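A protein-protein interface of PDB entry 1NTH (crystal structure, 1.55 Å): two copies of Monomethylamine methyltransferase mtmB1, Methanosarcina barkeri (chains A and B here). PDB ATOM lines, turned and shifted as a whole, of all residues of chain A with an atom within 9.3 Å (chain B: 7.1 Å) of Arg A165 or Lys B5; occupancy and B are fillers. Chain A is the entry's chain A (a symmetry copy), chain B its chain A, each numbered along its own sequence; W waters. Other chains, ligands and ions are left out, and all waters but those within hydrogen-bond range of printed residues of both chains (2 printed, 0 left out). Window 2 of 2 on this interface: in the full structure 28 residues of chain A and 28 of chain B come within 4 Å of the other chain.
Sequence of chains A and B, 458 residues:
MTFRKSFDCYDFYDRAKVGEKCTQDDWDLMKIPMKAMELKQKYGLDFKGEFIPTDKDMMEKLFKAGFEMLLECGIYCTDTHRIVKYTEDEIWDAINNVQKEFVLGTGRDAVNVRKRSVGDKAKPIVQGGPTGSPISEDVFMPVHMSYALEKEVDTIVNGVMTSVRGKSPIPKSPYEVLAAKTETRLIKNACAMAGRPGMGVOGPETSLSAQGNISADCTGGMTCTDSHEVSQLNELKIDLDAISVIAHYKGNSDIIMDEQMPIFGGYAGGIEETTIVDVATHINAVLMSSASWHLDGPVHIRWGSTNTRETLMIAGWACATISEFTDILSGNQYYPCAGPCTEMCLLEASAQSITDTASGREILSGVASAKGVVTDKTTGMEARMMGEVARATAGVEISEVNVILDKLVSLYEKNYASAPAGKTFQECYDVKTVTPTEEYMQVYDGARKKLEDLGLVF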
ATOM      1  N   GLU A 137       3.234  19.837  30.704  1.00  0.00           N
ATOM      2  CA  GLU A 137       4.070  19.885  29.511  1.00  0.00           C
ATOM      3  C   GLU A 137       4.039  21.229  28.782  1.00  0.00           C
ATOM      4  O   GLU A 137       5.088  21.736  28.376  1.00  0.00           O
ATOM      5  CB  GLU A 137       3.673  18.764  28.539  1.00  0.00           C
ATOM      6  CG  GLU A 137       4.655  18.589  27.383  1.00  0.00           C
ATOM      7  CD  GLU A 137       4.342  17.403  26.480  1.00  0.00           C
ATOM      8  OE1 GLU A 137       5.131  17.165  25.539  1.00  0.00           O
ATOM      9  OE2 GLU A 137       3.320  16.710  26.698  1.00  0.00           O
ATOM     10  N   ASP A 138       2.854  21.819  28.629  1.00  0.00           N
ATOM     11  CA  ASP A 138       2.760  23.083  27.903  1.00  0.00           C
ATOM     12  C   ASP A 138       3.430  24.295  28.545  1.00  0.00           C
ATOM     13  O   ASP A 138       3.540  25.343  27.913  1.00  0.00           O
ATOM     14  CB  ASP A 138       1.303  23.419  27.559  1.00  0.00           C
ATOM     15  CG  ASP A 138       0.401  23.481  28.774  1.00  0.00           C
ATOM     16  OD1 ASP A 138       0.903  23.675  29.901  1.00  0.00           O
ATOM     17  OD2 ASP A 138      -0.828  23.350  28.592  1.00  0.00           O
ATOM     18  N   MET A 161       8.127  16.105  34.235  1.00  0.00           N
ATOM     19  CA  MET A 161       7.181  16.294  33.136  1.00  0.00           C
ATOM     20  C   MET A 161       5.954  15.424  33.407  1.00  0.00           C
ATOM     21  O   MET A 161       6.083  14.209  33.538  1.00  0.00           O
ATOM     22  CB  MET A 161       7.803  15.858  31.801  1.00  0.00           C
ATOM     23  CG  MET A 161       9.046  16.637  31.375  1.00  0.00           C
ATOM     24  SD  MET A 161       9.641  16.162  29.721  1.00  0.00           S
ATOM     25  CE  MET A 161       8.430  17.014  28.676  1.00  0.00           C
ATOM     26  N   THR A 162       4.770  16.026  33.501  1.00  0.00           N
ATOM     27  CA  THR A 162       3.574  15.223  33.747  1.00  0.00           C
ATOM     28  C   THR A 162       3.230  14.430  32.493  1.00  0.00           C
ATOM     29  O   THR A 162       2.534  13.417  32.556  1.00  0.00           O
ATOM     30  CB  THR A 162       2.360  16.085  34.179  1.00  0.00           C
ATOM     31  OG1 THR A 162       2.113  17.113  33.212  1.00  0.00           O
ATOM     32  CG2 THR A 162       2.623  16.716  35.542  1.00  0.00           C
ATOM     33  N   SER A 163       3.720  14.895  31.347  1.00  0.00           N
ATOM     34  CA  SER A 163       3.504  14.196  30.089  1.00  0.00           C
ATOM     35  C   SER A 163       4.563  14.611  29.080  1.00  0.00           C
ATOM     36  O   SER A 163       5.179  15.671  29.205  1.00  0.00           O
ATOM     37  CB  SER A 163       2.107  14.491  29.513  1.00  0.00           C
ATOM     38  OG  SER A 163       1.993  15.825  29.037  1.00  0.00           O
ATOM     39  N   VAL A 164       4.799  13.745  28.102  1.00  0.00           N
ATOM     40  CA  VAL A 164       5.736  14.033  27.030  1.00  0.00           C
ATOM     41  C   VAL A 164       4.993  13.582  25.774  1.00  0.00           C
ATOM     42  O   VAL A 164       4.541  12.438  25.683  1.00  0.00           O
ATOM     43  CB  VAL A 164       7.086  13.288  27.217  1.00  0.00           C
ATOM     44  CG1 VAL A 164       6.885  11.778  27.200  1.00  0.00           C
ATOM     45  CG2 VAL A 164       8.062  13.731  26.141  1.00  0.00           C
ATOM     46  N   ARG A 165       4.843  14.495  24.818  1.00  0.00           N
ATOM     47  CA  ARG A 165       4.089  14.214  23.603  1.00  0.00           C
ATOM     48  C   ARG A 165       2.675  13.767  23.986  1.00  0.00           C
ATOM     49  O   ARG A 165       2.079  12.896  23.352  1.00  0.00           O
ATOM     50  CB  ARG A 165       4.801  13.164  22.737  1.00  0.00           C
ATOM     51  CG  ARG A 165       5.779  13.810  21.753  1.00  0.00           C
ATOM     52  CD  ARG A 165       6.694  12.817  21.050  1.00  0.00           C
ATOM     53  NE  ARG A 165       5.979  11.823  20.256  1.00  0.00           N
ATOM     54  CZ  ARG A 165       6.584  10.925  19.484  1.00  0.00           C
ATOM     55  NH1 ARG A 165       7.909  10.909  19.402  1.00  0.00           N
ATOM     56  NH2 ARG A 165       5.872  10.031  18.811  1.00  0.00           N
ATOM     57  N   GLY A 166       2.162  14.383  25.050  1.00  0.00           N
ATOM     58  CA  GLY A 166       0.818  14.100  25.527  1.00  0.00           C
ATOM     59  C   GLY A 166       0.587  12.772  26.223  1.00  0.00           C
ATOM     60  O   GLY A 166      -0.560  12.398  26.475  1.00  0.00           O
ATOM     61  N   LYS A 167       1.662  12.068  26.554  1.00  0.00           N
ATOM     62  CA  LYS A 167       1.549  10.769  27.211  1.00  0.00           C
ATOM     63  C   LYS A 167       2.316  10.726  28.528  1.00  0.00           C
ATOM     64  O   LYS A 167       3.363  11.357  28.671  1.00  0.00           O
ATOM     65  CB  LYS A 167       2.088   9.675  26.285  1.00  0.00           C
ATOM     66  CG  LYS A 167       1.328   9.522  24.976  1.00  0.00           C
ATOM     67  CD  LYS A 167      -0.030   8.871  25.188  1.00  0.00           C
ATOM     68  CE  LYS A 167      -0.750   8.666  23.865  1.00  0.00           C
ATOM     69  NZ  LYS A 167      -2.044   7.958  24.051  1.00  0.00           N
ATOM     70  N   SER A 168       1.795   9.973  29.492  1.00  0.00           N
ATOM     71  CA  SER A 168       2.460   9.839  30.784  1.00  0.00           C
ATOM     72  C   SER A 168       3.746   9.038  30.615  1.00  0.00           C
ATOM     73  O   SER A 168       3.768   8.026  29.917  1.00  0.00           O
ATOM     74  CB  SER A 168       1.549   9.125  31.784  1.00  0.00           C
ATOM     75  OG  SER A 168       0.365   9.870  32.004  1.00  0.00           O
ATOM     76  N   PRO A 169       4.839   9.485  31.256  1.00  0.00           N
ATOM     77  CA  PRO A 169       6.139   8.809  31.179  1.00  0.00           C
ATOM     78  C   PRO A 169       6.187   7.582  32.091  1.00  0.00           C
ATOM     79  O   PRO A 169       7.010   7.503  33.006  1.00  0.00           O
ATOM     80  CB  PRO A 169       7.108   9.898  31.619  1.00  0.00           C
ATOM     81  CG  PRO A 169       6.319  10.611  32.670  1.00  0.00           C
ATOM     82  CD  PRO A 169       4.942  10.733  32.034  1.00  0.00           C
ATOM     83  N   PRO A 174       8.744   3.360  26.694  1.00  0.00           N
ATOM     84  CA  PRO A 174       9.635   4.213  25.900  1.00  0.00           C
ATOM     85  C   PRO A 174       9.427   5.689  26.233  1.00  0.00           C
ATOM     86  O   PRO A 174      10.323   6.511  26.036  1.00  0.00           O
ATOM     87  CB  PRO A 174       9.259   3.867  24.460  1.00  0.00           C
ATOM     88  CG  PRO A 174       7.809   3.426  24.576  1.00  0.00           C
ATOM     89  CD  PRO A 174       7.848   2.578  25.823  1.00  0.00           C
ATOM     90  N   TYR A 175       8.245   6.024  26.745  1.00  0.00           N
ATOM     91  CA  TYR A 175       7.961   7.406  27.113  1.00  0.00           C
ATOM     92  C   TYR A 175       8.839   7.867  28.271  1.00  0.00           C
ATOM     93  O   TYR A 175       9.146   9.054  28.389  1.00  0.00           O
ATOM     94  CB  TYR A 175       6.487   7.579  27.489  1.00  0.00           C
ATOM     95  CG  TYR A 175       5.548   7.448  26.317  1.00  0.00           C
ATOM     96  CD1 TYR A 175       4.750   6.313  26.161  1.00  0.00           C
ATOM     97  CD2 TYR A 175       5.454   8.458  25.359  1.00  0.00           C
ATOM     98  CE1 TYR A 175       3.878   6.194  25.087  1.00  0.00           C
ATOM     99  CE2 TYR A 175       4.581   8.346  24.278  1.00  0.00           C
ATOM    100  CZ  TYR A 175       3.797   7.212  24.152  1.00  0.00           C
ATOM    101  OH  TYR A 175       2.924   7.101  23.095  1.00  0.00           O
ATOM    102  N   LEU A 178      12.098   8.792  26.660  1.00  0.00           N
ATOM    103  CA  LEU A 178      11.910  10.057  25.956  1.00  0.00           C
ATOM    104  C   LEU A 178      11.904  11.223  26.946  1.00  0.00           C
ATOM    105  O   LEU A 178      12.552  12.248  26.715  1.00  0.00           O
ATOM    106  CB  LEU A 178      10.594  10.039  25.161  1.00  0.00           C
ATOM    107  CG  LEU A 178      10.239  11.324  24.403  1.00  0.00           C
ATOM    108  CD1 LEU A 178      11.334  11.644  23.390  1.00  0.00           C
ATOM    109  CD2 LEU A 178       8.896  11.154  23.701  1.00  0.00           C
ATOM    110  N   ALA A 179      11.180  11.066  28.051  1.00  0.00           N
ATOM    111  CA  ALA A 179      11.107  12.122  29.057  1.00  0.00           C
ATOM    112  C   ALA A 179      12.457  12.375  29.721  1.00  0.00           C
ATOM    113  O   ALA A 179      12.814  13.524  29.988  1.00  0.00           O
ATOM    114  CB  ALA A 179      10.055  11.773  30.121  1.00  0.00           C
ATOM    115  N   THR A 182      14.443  14.334  27.116  1.00  0.00           N
ATOM    116  CA  THR A 182      13.743  15.587  26.835  1.00  0.00           C
ATOM    117  C   THR A 182      13.741  16.600  27.977  1.00  0.00           C
ATOM    118  O   THR A 182      13.904  17.804  27.755  1.00  0.00           O
ATOM    119  CB  THR A 182      12.285  15.293  26.423  1.00  0.00           C
ATOM    120  OG1 THR A 182      12.286  14.442  25.271  1.00  0.00           O
ATOM    121  CG2 THR A 182      11.540  16.581  26.096  1.00  0.00           C
ATOM    122  N   LEU A 186      14.917  20.380  27.227  1.00  0.00           N
ATOM    123  CA  LEU A 186      14.008  21.520  27.305  1.00  0.00           C
ATOM    124  C   LEU A 186      14.469  22.545  28.339  1.00  0.00           C
ATOM    125  O   LEU A 186      14.394  23.753  28.106  1.00  0.00           O
ATOM    126  CB  LEU A 186      12.593  21.057  27.665  1.00  0.00           C
ATOM    127  CG  LEU A 186      11.846  20.218  26.630  1.00  0.00           C
ATOM    128  CD1 LEU A 186      10.499  19.789  27.196  1.00  0.00           C
ATOM    129  CD2 LEU A 186      11.660  21.031  25.352  1.00  0.00           C
ATOM    130  N   THR B   2      -5.569   7.438   4.960  1.00  0.00           N
ATOM    131  CA  THR B   2      -4.109   7.548   5.223  1.00  0.00           C
ATOM    132  C   THR B   2      -3.845   7.214   6.687  1.00  0.00           C
ATOM    133  O   THR B   2      -4.775   6.937   7.444  1.00  0.00           O
ATOM    134  CB  THR B   2      -3.603   8.977   4.918  1.00  0.00           C
ATOM    135  OG1 THR B   2      -2.174   9.019   5.038  1.00  0.00           O
ATOM    136  CG2 THR B   2      -4.222   9.979   5.882  1.00  0.00           C
ATOM    137  N   PHE B   3      -2.577   7.233   7.085  1.00  0.00           N
ATOM    138  CA  PHE B   3      -2.204   6.927   8.462  1.00  0.00           C
ATOM    139  C   PHE B   3      -2.296   8.160   9.360  1.00  0.00           C
ATOM    140  O   PHE B   3      -2.218   9.291   8.879  1.00  0.00           O
ATOM    141  CB  PHE B   3      -0.783   6.345   8.488  1.00  0.00           C
ATOM    142  CG  PHE B   3       0.238   7.185   7.764  1.00  0.00           C
ATOM    143  CD1 PHE B   3       0.993   8.136   8.447  1.00  0.00           C
ATOM    144  CD2 PHE B   3       0.445   7.023   6.396  1.00  0.00           C
ATOM    145  CE1 PHE B   3       1.942   8.918   7.773  1.00  0.00           C
ATOM    146  CE2 PHE B   3       1.389   7.797   5.714  1.00  0.00           C
ATOM    147  CZ  PHE B   3       2.139   8.745   6.407  1.00  0.00           C
ATOM    148  N   ARG B   4      -2.476   7.952  10.661  1.00  0.00           N
ATOM    149  CA  ARG B   4      -2.566   9.079  11.582  1.00  0.00           C
ATOM    150  C   ARG B   4      -1.198   9.740  11.710  1.00  0.00           C
ATOM    151  O   ARG B   4      -1.068  10.957  11.597  1.00  0.00           O
ATOM    152  CB  ARG B   4      -3.062   8.629  12.963  1.00  0.00           C
ATOM    153  CG  ARG B   4      -3.378   9.804  13.884  1.00  0.00           C
ATOM    154  CD  ARG B   4      -4.119   9.389  15.151  1.00  0.00           C
ATOM    155  NE  ARG B   4      -3.247   8.773  16.147  1.00  0.00           N
ATOM    156  CZ  ARG B   4      -3.165   9.177  17.412  1.00  0.00           C
ATOM    157  NH1 ARG B   4      -3.901  10.197  17.835  1.00  0.00           N
ATOM    158  NH2 ARG B   4      -2.350   8.561  18.259  1.00  0.00           N
ATOM    159  N   LYS B   5      -0.175   8.925  11.941  1.00  0.00           N
ATOM    160  CA  LYS B   5       1.188   9.423  12.064  1.00  0.00           C
ATOM    161  C   LYS B   5       2.138   8.289  11.718  1.00  0.00           C
ATOM    162  O   LYS B   5       1.762   7.117  11.802  1.00  0.00           O
ATOM    163  CB  LYS B   5       1.465   9.901  13.495  1.00  0.00           C
ATOM    164  CG  LYS B   5       1.401   8.799  14.549  1.00  0.00           C
ATOM    165  CD  LYS B   5       1.768   9.312  15.941  1.00  0.00           C
ATOM    166  CE  LYS B   5       3.241   9.700  16.046  1.00  0.00           C
ATOM    167  NZ  LYS B   5       4.151   8.530  15.857  1.00  0.00           N
ATOM    168  N   SER B   6       3.359   8.624  11.313  1.00  0.00           N
ATOM    169  CA  SER B   6       4.325   7.584  10.995  1.00  0.00           C
ATOM    170  C   SER B   6       4.482   6.754  12.262  1.00  0.00           C
ATOM    171  O   SER B   6       4.666   7.294  13.353  1.00  0.00           O
ATOM    172  CB  SER B   6       5.667   8.192  10.580  1.00  0.00           C
ATOM    173  OG  SER B   6       5.550   8.858   9.332  1.00  0.00           O
ATOM    174  N   PHE B   7       4.404   5.440  12.113  1.00  0.00           N
ATOM    175  CA  PHE B   7       4.499   4.539  13.251  1.00  0.00           C
ATOM    176  C   PHE B   7       5.876   4.517  13.913  1.00  0.00           C
ATOM    177  O   PHE B   7       6.900   4.552  13.236  1.00  0.00           O
ATOM    178  CB  PHE B   7       4.138   3.121  12.804  1.00  0.00           C
ATOM    179  CG  PHE B   7       3.965   2.158  13.939  1.00  0.00           C
ATOM    180  CD1 PHE B   7       2.719   1.984  14.532  1.00  0.00           C
ATOM    181  CD2 PHE B   7       5.051   1.450  14.435  1.00  0.00           C
ATOM    182  CE1 PHE B   7       2.563   1.115  15.608  1.00  0.00           C
ATOM    183  CE2 PHE B   7       4.907   0.581  15.510  1.00  0.00           C
ATOM    184  CZ  PHE B   7       3.657   0.413  16.097  1.00  0.00           C
ATOM    185  N   ASP B   8       5.890   4.467  15.242  1.00  0.00           N
ATOM    186  CA  ASP B   8       7.142   4.386  15.987  1.00  0.00           C
ATOM    187  C   ASP B   8       6.967   3.568  17.264  1.00  0.00           C
ATOM    188  O   ASP B   8       5.862   3.114  17.577  1.00  0.00           O
ATOM    189  CB  ASP B   8       7.703   5.782  16.310  1.00  0.00           C
ATOM    190  CG  ASP B   8       6.742   6.643  17.105  1.00  0.00           C
ATOM    191  OD1 ASP B   8       5.977   6.095  17.924  1.00  0.00           O
ATOM    192  OD2 ASP B   8       6.770   7.883  16.920  1.00  0.00           O
ATOM    193  N   CYS B   9       8.065   3.374  17.989  1.00  0.00           N
ATOM    194  CA  CYS B   9       8.062   2.592  19.222  1.00  0.00           C
ATOM    195  C   CYS B   9       7.045   3.076  20.255  1.00  0.00           C
ATOM    196  O   CYS B   9       6.556   2.287  21.066  1.00  0.00           O
ATOM    197  CB  CYS B   9       9.466   2.581  19.842  1.00  0.00           C
ATOM    198  SG  CYS B   9      10.167   4.226  20.162  1.00  0.00           S
ATOM    199  N   TYR B  10       6.728   4.367  20.229  1.00  0.00           N
ATOM    200  CA  TYR B  10       5.769   4.916  21.177  1.00  0.00           C
ATOM    201  C   TYR B  10       4.368   4.422  20.840  1.00  0.00           C
ATOM    202  O   TYR B  10       3.591   4.084  21.736  1.00  0.00           O
ATOM    203  CB  TYR B  10       5.829   6.444  21.162  1.00  0.00           C
ATOM    204  CG  TYR B  10       7.217   6.958  21.463  1.00  0.00           C
ATOM    205  CD1 TYR B  10       8.058   7.393  20.439  1.00  0.00           C
ATOM    206  CD2 TYR B  10       7.713   6.948  22.765  1.00  0.00           C
ATOM    207  CE1 TYR B  10       9.363   7.801  20.703  1.00  0.00           C
ATOM    208  CE2 TYR B  10       9.020   7.355  23.041  1.00  0.00           C
ATOM    209  CZ  TYR B  10       9.838   7.776  22.007  1.00  0.00           C
ATOM    210  OH  TYR B  10      11.133   8.162  22.273  1.00  0.00           O
ATOM    211  N   ASP B  11       4.048   4.378  19.551  1.00  0.00           N
ATOM    212  CA  ASP B  11       2.743   3.885  19.121  1.00  0.00           C
ATOM    213  C   ASP B  11       2.663   2.404  19.463  1.00  0.00           C
ATOM    214  O   ASP B  11       1.603   1.897  19.830  1.00  0.00           O
ATOM    215  CB  ASP B  11       2.559   4.045  17.612  1.00  0.00           C
ATOM    216  CG  ASP B  11       2.557   5.488  17.171  1.00  0.00           C
ATOM    217  OD1 ASP B  11       1.761   6.276  17.723  1.00  0.00           O
ATOM    218  OD2 ASP B  11       3.348   5.832  16.267  1.00  0.00           O
ATOM    219  N   ARG B  15      -0.336   0.631  21.682  1.00  0.00           N
ATOM    220  CA  ARG B  15      -1.146  -0.475  21.187  1.00  0.00           C
ATOM    221  C   ARG B  15      -0.934  -1.779  21.942  1.00  0.00           C
ATOM    222  O   ARG B  15      -1.868  -2.570  22.093  1.00  0.00           O
ATOM    223  CB  ARG B  15      -0.881  -0.673  19.693  1.00  0.00           C
ATOM    224  CG  ARG B  15      -1.202   0.572  18.886  1.00  0.00           C
ATOM    225  CD  ARG B  15      -0.978   0.396  17.399  1.00  0.00           C
ATOM    226  NE  ARG B  15      -1.124   1.681  16.717  1.00  0.00           N
ATOM    227  CZ  ARG B  15      -1.092   1.846  15.400  1.00  0.00           C
ATOM    228  NH1 ARG B  15      -0.923   0.802  14.599  1.00  0.00           N
ATOM    229  NH2 ARG B  15      -1.216   3.063  14.885  1.00  0.00           N
ATOM    230  N   GLU B  90       0.206   2.461   7.148  1.00  0.00           N
ATOM    231  CA  GLU B  90       1.323   2.662   8.066  1.00  0.00           C
ATOM    232  C   GLU B  90       2.525   1.856   7.596  1.00  0.00           C
ATOM    233  O   GLU B  90       3.661   2.328   7.664  1.00  0.00           O
ATOM    234  CB  GLU B  90       0.944   2.240   9.490  1.00  0.00           C
ATOM    235  CG  GLU B  90      -0.167   3.076  10.098  1.00  0.00           C
ATOM    236  CD  GLU B  90      -0.610   2.578  11.463  1.00  0.00           C
ATOM    237  OE1 GLU B  90      -0.434   1.374  11.751  1.00  0.00           O
ATOM    238  OE2 GLU B  90      -1.153   3.394  12.238  1.00  0.00           O
ATOM    239  N   ASP B  93       4.104   3.589   4.575  1.00  0.00           N
ATOM    240  CA  ASP B  93       4.805   4.810   4.961  1.00  0.00           C
ATOM    241  C   ASP B  93       6.210   4.438   5.435  1.00  0.00           C
ATOM    242  O   ASP B  93       7.178   5.131   5.137  1.00  0.00           O
ATOM    243  CB  ASP B  93       4.040   5.532   6.076  1.00  0.00           C
ATOM    244  CG  ASP B  93       4.815   6.708   6.660  1.00  0.00           C
ATOM    245  OD1 ASP B  93       5.153   6.650   7.858  1.00  0.00           O
ATOM    246  OD2 ASP B  93       5.082   7.686   5.923  1.00  0.00           O
ATOM    247  N   LYS B 250      17.049   6.120  19.131  1.00  0.00           N
ATOM    248  CA  LYS B 250      16.487   7.206  18.331  1.00  0.00           C
ATOM    249  C   LYS B 250      16.816   8.553  18.956  1.00  0.00           C
ATOM    250  O   LYS B 250      17.194   9.495  18.255  1.00  0.00           O
ATOM    251  CB  LYS B 250      14.966   7.059  18.229  1.00  0.00           C
ATOM    252  CG  LYS B 250      14.507   5.884  17.370  1.00  0.00           C
ATOM    253  CD  LYS B 250      13.034   5.565  17.600  1.00  0.00           C
ATOM    254  CE  LYS B 250      12.111   6.697  17.163  1.00  0.00           C
ATOM    255  NZ  LYS B 250      12.152   6.915  15.687  1.00  0.00           N
HETATM  256  O   HOH W   1       3.526   8.092  18.754  1.00  0.00           O
HETATM  257  O   HOH W   2       9.500   9.132  17.477  1.00  0.00           O
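NZ of Lys B5 lies within salt-bridge range of OD2 of Asp B8 (2.9 Å). NZ of Lys B5 lies within salt-bridge range of OD2 of Asp B11, 2.8 Å away. The backbone NH (N) of Tyr B10 lies within hydrogen-bond range of the side-chain carboxylate (OD1) of Asp B8, at 3.0 Å. The side-chain carboxylate of Asp B8 sits at hydrogen-bond distance from the backbone NH of Asp B11 (3.1 Å). OE1 of Glu A137 lies within hydrogen-bond range of N of Arg A165 (2.8 Å). OG1 of Thr A182 sits at hydrogen-bond distance from O of Leu A178.
Ser A163 touches none of the printed residues of chain B. Val A164 touches none of the printed residues of chain B. Of chain B, only Lys B5 (3.7 Å), Asp B8 (3.0 Å) and Tyr B10 (3.7 Å) come within 4 Å of Arg A165. Printed residues of chain B within 4 Å of Tyr A175: Tyr B10 (3.4 Å). Of chain A, only Arg A165 comes within 4 Å of Lys B5. No residue of chain A comes within 4 Å of Ser B6. Of the printed residues of chain A, Asp B8 touches Arg A165. Of the printed residues of chain A, Cys B9 touches Pro A174. Printed residues of chain A within 4 Å of Tyr B10: Arg A165, Pro A174, Tyr A175 and Leu A178. The nearest residue of chain B that does not touch Arg A165 is Asp B11 (5.5 Å). The nearest printed residue of chain A that does not touch Lys B5 is Tyr A175 (7.5 Å).
Of the 14 printed residues of chain B, 4 touch a printed residue of chain A. Printed residues of chain B that touch a printed residue of chain A: Lys B5, Asp B8, Cys B9 and Tyr B10. Hydrophobic or aromatic side chains of chain B that line the printed part of chain A: Tyr B10. Hydrophobic or aromatic side chains of chain A that line the printed part of chain B: Pro A174, Tyr A175 and Leu A178. Among the printed residues, 7 pairs touch across the chains.
Water W1 lies within hydrogen-bond range of OD1 of Asp B11 (2.7 Å), NZ of Lys B5 (3.0 Å), NH2 of Arg A165 (3.0 Å) and OD1 of Asp B8 (3.3 Å). Water W2 lies within hydrogen-bond range of OD2 of Asp B8 (3.1 Å) and NH1 of Arg A165 (3.1 Å).
Among the printed residues, merely in contact across the chains: Pro A174 with Tyr B10 (3.4 Å), Leu A178 with Tyr B10 (3.5 Å), Arg A165 with Tyr B10 (3.7 Å), Arg A165 with Lys B5 (3.7 Å) and Pro A174 with Cys B9 (3.9 Å).
The side-chain carboxylate of Asp B8 lies within salt-bridge range of the guanidinium group of Arg A165, at 3.0 Å. The backbone carbonyl oxygen (O) of Tyr B10 lies within hydrogen-bond range of the side-chain hydroxyl (OH) of Tyr A175 (3.4 Å).
No position is printed for both chains.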
